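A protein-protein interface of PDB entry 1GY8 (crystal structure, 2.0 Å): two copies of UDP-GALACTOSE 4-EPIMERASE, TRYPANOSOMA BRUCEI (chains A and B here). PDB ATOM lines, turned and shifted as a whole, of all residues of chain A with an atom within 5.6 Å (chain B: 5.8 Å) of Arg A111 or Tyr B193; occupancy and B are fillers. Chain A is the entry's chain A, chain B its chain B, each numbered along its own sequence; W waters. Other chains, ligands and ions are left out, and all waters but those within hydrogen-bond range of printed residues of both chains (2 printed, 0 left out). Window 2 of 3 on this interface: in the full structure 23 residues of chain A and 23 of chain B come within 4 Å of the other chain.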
ATOM      1  N   GLY A 107       7.403   7.829  -3.829  1.00  0.00           N
ATOM      2  CA  GLY A 107       7.324   8.774  -2.730  1.00  0.00           C
ATOM      3  C   GLY A 107       6.015   9.537  -2.712  1.00  0.00           C
ATOM      4  O   GLY A 107       5.455   9.795  -1.650  1.00  0.00           O
ATOM      5  N   GLU A 108       5.522   9.899  -3.892  1.00  0.00           N
ATOM      6  CA  GLU A 108       4.271  10.633  -3.998  1.00  0.00           C
ATOM      7  C   GLU A 108       3.056   9.757  -3.702  1.00  0.00           C
ATOM      8  O   GLU A 108       2.039  10.249  -3.205  1.00  0.00           O
ATOM      9  CB  GLU A 108       4.113  11.245  -5.394  1.00  0.00           C
ATOM     10  CG  GLU A 108       2.748  11.906  -5.591  1.00  0.00           C
ATOM     11  CD  GLU A 108       2.438  12.263  -7.037  1.00  0.00           C
ATOM     12  OE1 GLU A 108       2.937  11.564  -7.950  1.00  0.00           O
ATOM     13  OE2 GLU A 108       1.673  13.231  -7.256  1.00  0.00           O
ATOM     14  N   SER A 109       3.144   8.463  -4.006  1.00  0.00           N
ATOM     15  CA  SER A 109       2.015   7.571  -3.759  1.00  0.00           C
ATOM     16  C   SER A 109       1.715   7.452  -2.265  1.00  0.00           C
ATOM     17  O   SER A 109       0.565   7.272  -1.871  1.00  0.00           O
ATOM     18  CB  SER A 109       2.271   6.183  -4.363  1.00  0.00           C
ATOM     19  OG  SER A 109       3.229   5.444  -3.632  1.00  0.00           O
ATOM     20  N   VAL A 110       2.753   7.555  -1.438  1.00  0.00           N
ATOM     21  CA  VAL A 110       2.586   7.471   0.011  1.00  0.00           C
ATOM     22  C   VAL A 110       1.837   8.700   0.531  1.00  0.00           C
ATOM     23  O   VAL A 110       0.993   8.588   1.415  1.00  0.00           O
ATOM     24  CB  VAL A 110       3.956   7.355   0.729  1.00  0.00           C
ATOM     25  CG1 VAL A 110       3.775   7.436   2.247  1.00  0.00           C
ATOM     26  CG2 VAL A 110       4.618   6.031   0.357  1.00  0.00           C
ATOM     27  N   ARG A 111       2.133   9.866  -0.043  1.00  0.00           N
ATOM     28  CA  ARG A 111       1.500  11.120   0.360  1.00  0.00           C
ATOM     29  C   ARG A 111       0.110  11.316  -0.241  1.00  0.00           C
ATOM     30  O   ARG A 111      -0.729  12.007   0.339  1.00  0.00           O
ATOM     31  CB  ARG A 111       2.384  12.314  -0.040  1.00  0.00           C
ATOM     32  CG  ARG A 111       3.755  12.327   0.618  1.00  0.00           C
ATOM     33  CD  ARG A 111       4.585  13.560   0.230  1.00  0.00           C
ATOM     34  NE  ARG A 111       5.343  13.407  -1.016  1.00  0.00           N
ATOM     35  CZ  ARG A 111       4.972  13.902  -2.195  1.00  0.00           C
ATOM     36  NH1 ARG A 111       3.840  14.593  -2.304  1.00  0.00           N
ATOM     37  NH2 ARG A 111       5.740  13.721  -3.267  1.00  0.00           N
ATOM     38  N   ASP A 112      -0.133  10.718  -1.404  1.00  0.00           N
ATOM     39  CA  ASP A 112      -1.418  10.865  -2.075  1.00  0.00           C
ATOM     40  C   ASP A 112      -1.853   9.539  -2.710  1.00  0.00           C
ATOM     41  O   ASP A 112      -1.834   9.389  -3.933  1.00  0.00           O
ATOM     42  CB  ASP A 112      -1.303  11.957  -3.140  1.00  0.00           C
ATOM     43  CG  ASP A 112      -2.646  12.365  -3.710  1.00  0.00           C
ATOM     44  OD1 ASP A 112      -3.675  11.790  -3.295  1.00  0.00           O
ATOM     45  OD2 ASP A 112      -2.673  13.264  -4.573  1.00  0.00           O
ATOM     46  N   PRO A 113      -2.267   8.566  -1.877  1.00  0.00           N
ATOM     47  CA  PRO A 113      -2.719   7.225  -2.273  1.00  0.00           C
ATOM     48  C   PRO A 113      -3.852   7.187  -3.293  1.00  0.00           C
ATOM     49  O   PRO A 113      -3.787   6.446  -4.271  1.00  0.00           O
ATOM     50  CB  PRO A 113      -3.164   6.595  -0.956  1.00  0.00           C
ATOM     51  CG  PRO A 113      -2.412   7.346   0.082  1.00  0.00           C
ATOM     52  CD  PRO A 113      -2.439   8.758  -0.426  1.00  0.00           C
ATOM     53  N   LEU A 114      -4.893   7.976  -3.057  1.00  0.00           N
ATOM     54  CA  LEU A 114      -6.049   7.985  -3.942  1.00  0.00           C
ATOM     55  C   LEU A 114      -5.744   8.345  -5.388  1.00  0.00           C
ATOM     56  O   LEU A 114      -6.426   7.878  -6.304  1.00  0.00           O
ATOM     57  CB  LEU A 114      -7.138   8.906  -3.377  1.00  0.00           C
ATOM     58  CG  LEU A 114      -7.682   8.484  -2.000  1.00  0.00           C
ATOM     59  CD1 LEU A 114      -8.733   9.486  -1.537  1.00  0.00           C
ATOM     60  CD2 LEU A 114      -8.290   7.081  -2.068  1.00  0.00           C
ATOM     61  N   LYS A 115      -4.731   9.178  -5.596  1.00  0.00           N
ATOM     62  CA  LYS A 115      -4.342   9.563  -6.945  1.00  0.00           C
ATOM     63  C   LYS A 115      -3.808   8.326  -7.667  1.00  0.00           C
ATOM     64  O   LYS A 115      -4.053   8.130  -8.864  1.00  0.00           O
ATOM     65  CB  LYS A 115      -3.258  10.647  -6.898  1.00  0.00           C
ATOM     66  CG  LYS A 115      -2.705  11.035  -8.260  1.00  0.00           C
ATOM     67  CD  LYS A 115      -1.662  12.138  -8.145  1.00  0.00           C
ATOM     68  CE  LYS A 115      -1.058  12.482  -9.504  1.00  0.00           C
ATOM     69  NZ  LYS A 115      -0.077  13.599  -9.414  1.00  0.00           N
ATOM     70  N   LEU B 132     -12.737  12.942   1.570  1.00  0.00           N
ATOM     71  CA  LEU B 132     -11.634  13.892   1.535  1.00  0.00           C
ATOM     72  C   LEU B 132     -12.146  15.261   1.092  1.00  0.00           C
ATOM     73  O   LEU B 132     -11.861  16.283   1.715  1.00  0.00           O
ATOM     74  CB  LEU B 132     -10.571  13.390   0.564  1.00  0.00           C
ATOM     75  CG  LEU B 132      -9.126  13.710   0.922  1.00  0.00           C
ATOM     76  CD1 LEU B 132      -8.839  13.195   2.329  1.00  0.00           C
ATOM     77  CD2 LEU B 132      -8.195  13.065  -0.098  1.00  0.00           C
ATOM     78  N   ASP B 188      -4.070   3.189   4.022  1.00  0.00           N
ATOM     79  CA  ASP B 188      -3.181   4.208   3.470  1.00  0.00           C
ATOM     80  C   ASP B 188      -3.747   5.622   3.584  1.00  0.00           C
ATOM     81  O   ASP B 188      -2.993   6.596   3.598  1.00  0.00           O
ATOM     82  CB  ASP B 188      -2.851   3.900   2.008  1.00  0.00           C
ATOM     83  CG  ASP B 188      -2.118   2.582   1.839  1.00  0.00           C
ATOM     84  OD1 ASP B 188      -1.551   2.071   2.828  1.00  0.00           O
ATOM     85  OD2 ASP B 188      -2.100   2.059   0.709  1.00  0.00           O
ATOM     86  N   CYS B 189      -5.071   5.736   3.658  1.00  0.00           N
ATOM     87  CA  CYS B 189      -5.710   7.040   3.791  1.00  0.00           C
ATOM     88  C   CYS B 189      -5.574   7.568   5.215  1.00  0.00           C
ATOM     89  O   CYS B 189      -5.660   8.767   5.445  1.00  0.00           O
ATOM     90  CB  CYS B 189      -7.188   6.952   3.417  1.00  0.00           C
ATOM     91  SG  CYS B 189      -7.492   6.782   1.637  1.00  0.00           S
ATOM     92  N   ALA B 190      -5.375   6.669   6.171  1.00  0.00           N
ATOM     93  CA  ALA B 190      -5.218   7.070   7.563  1.00  0.00           C
ATOM     94  C   ALA B 190      -3.906   7.823   7.665  1.00  0.00           C
ATOM     95  O   ALA B 190      -3.855   8.966   8.120  1.00  0.00           O
ATOM     96  CB  ALA B 190      -5.190   5.839   8.468  1.00  0.00           C
ATOM     97  N   GLU B 191      -2.859   7.152   7.205  1.00  0.00           N
ATOM     98  CA  GLU B 191      -1.499   7.660   7.197  1.00  0.00           C
ATOM     99  C   GLU B 191      -1.358   8.958   6.401  1.00  0.00           C
ATOM    100  O   GLU B 191      -0.696   9.892   6.837  1.00  0.00           O
ATOM    101  CB  GLU B 191      -0.584   6.582   6.599  1.00  0.00           C
ATOM    102  CG  GLU B 191       0.893   6.924   6.554  1.00  0.00           C
ATOM    103  CD  GLU B 191       1.533   6.918   7.932  1.00  0.00           C
ATOM    104  OE1 GLU B 191       1.357   5.913   8.662  1.00  0.00           O
ATOM    105  OE2 GLU B 191       2.215   7.911   8.282  1.00  0.00           O
ATOM    106  N   ALA B 192      -2.000   9.011   5.239  1.00  0.00           N
ATOM    107  CA  ALA B 192      -1.919  10.158   4.344  1.00  0.00           C
ATOM    108  C   ALA B 192      -2.845  11.340   4.608  1.00  0.00           C
ATOM    109  O   ALA B 192      -2.421  12.484   4.488  1.00  0.00           O
ATOM    110  CB  ALA B 192      -2.115   9.682   2.904  1.00  0.00           C
ATOM    111  N   TYR B 193      -4.102  11.076   4.951  1.00  0.00           N
ATOM    112  CA  TYR B 193      -5.062  12.155   5.169  1.00  0.00           C
ATOM    113  C   TYR B 193      -5.665  12.234   6.566  1.00  0.00           C
ATOM    114  O   TYR B 193      -6.504  13.101   6.829  1.00  0.00           O
ATOM    115  CB  TYR B 193      -6.205  12.032   4.169  1.00  0.00           C
ATOM    116  CG  TYR B 193      -5.784  11.617   2.775  1.00  0.00           C
ATOM    117  CD1 TYR B 193      -5.037  12.474   1.957  1.00  0.00           C
ATOM    118  CD2 TYR B 193      -6.166  10.382   2.260  1.00  0.00           C
ATOM    119  CE1 TYR B 193      -4.690  12.108   0.657  1.00  0.00           C
ATOM    120  CE2 TYR B 193      -5.829  10.005   0.968  1.00  0.00           C
ATOM    121  CZ  TYR B 193      -5.098  10.868   0.170  1.00  0.00           C
ATOM    122  OH  TYR B 193      -4.803  10.493  -1.120  1.00  0.00           O
ATOM    123  N   GLY B 194      -5.260  11.334   7.455  1.00  0.00           N
ATOM    124  CA  GLY B 194      -5.805  11.352   8.801  1.00  0.00           C
ATOM    125  C   GLY B 194      -7.208  10.765   8.893  1.00  0.00           C
ATOM    126  O   GLY B 194      -7.932  11.009   9.859  1.00  0.00           O
ATOM    127  N   ILE B 195      -7.611  10.003   7.882  1.00  0.00           N
ATOM    128  CA  ILE B 195      -8.925   9.378   7.916  1.00  0.00           C
ATOM    129  C   ILE B 195      -8.882   8.230   8.923  1.00  0.00           C
ATOM    130  O   ILE B 195      -7.973   7.397   8.889  1.00  0.00           O
ATOM    131  CB  ILE B 195      -9.329   8.847   6.514  1.00  0.00           C
ATOM    132  CG1 ILE B 195      -9.768  10.027   5.642  1.00  0.00           C
ATOM    133  CG2 ILE B 195     -10.442   7.803   6.630  1.00  0.00           C
ATOM    134  CD1 ILE B 195     -10.246   9.645   4.261  1.00  0.00           C
HETATM  135  O   HOH W   1      -0.431  13.293   2.685  1.00  0.00           O
HETATM  136  O   HOH W   2      -0.528   6.358   2.402  1.00  0.00           O
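Of the 9 printed residues of chain A, 5 touch a printed residue of chain B.
Hydrophobic or aromatic side chains of chain A that line the printed part of chain B: Pro A113 and Leu A114.
Among the printed residues, 10 pairs touch across the chains.
Among the printed residues, no Asp or Glu carboxylate lies within 4 Å of a Lys or Arg side-chain nitrogen of the other chain.
Val A110 touches Ala B192.
Ala B192 touches Arg A111.
CE1 of Tyr B193 touches O of Arg A111 (3.98 Å).
O of Asp B188 touches CG of Pro A113, at 3.6 Å.
Ala B192 touches Pro A113 (CB to CD, 3.5 Å).
Leu B132 touches Leu A114.
Cys B189 touches Leu A114 (SG to CD2, 3.8 Å).
The backbone carbonyl oxygen (O) of Cys B189 is in hydrogen-bond range of the backbone NH (N) of Gly B194 (3.3 Å).
N of Ile B195 sits at hydrogen-bond distance from O of Cys B189, at 3.4 Å.
OH of Tyr B193 is in hydrogen-bond range of OD1 of Asp A112, 2.8 Å away.
The side-chain hydroxyl of Tyr B193 sits at hydrogen-bond distance from the backbone NH of Leu A114 (3.2 Å).
N of Pro A113 lies close to OH of Tyr B193 (3.3 Å).
No position is printed for both chains.
Of the 10 pairs that touch across the chains among the printed residues, none has its exchanged pair printed and touching as well.
Water W1 bridges O of Arg A111 and O of Ala B192.
Water W2 lies within hydrogen-bond range of the backbone carbonyl oxygen (O) of Asp B188 and the backbone carbonyl oxygen (O) of Val A110.
Of the printed residues of chain B, Val A110 touches Ala B192 (3.6 Å).
Of chain B, only Ala B192 and Tyr B193 come within 4 Å of Arg A111.
Of the printed residues of chain B, Asp A112 touches Tyr B193 (2.8 Å).
Lys A115 touches none of the printed residues of chain B.
Printed residues of chain A within 4 Å of Leu B132: Leu A114 (3.9 Å).
Of the printed residues of chain A, Cys B189 touches Leu A114 (3.8 Å).
Of the printed residues of chain A, Ala B192 touches Val A110 (3.6 Å), Arg A111 (3.7 Å) and Pro A113 (3.5 Å).
Tyr B193 touches four residues of chain A.
The nearest printed residue of chain B that does not touch Arg A111 is Asp B188 (6.7 Å).
The nearest residue of chain A that does not touch Tyr B193 is Lys A115 (4.7 Å).
The nearest printed residue of chain A that does not touch Asp B188 is Val A110 (5.0 Å).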
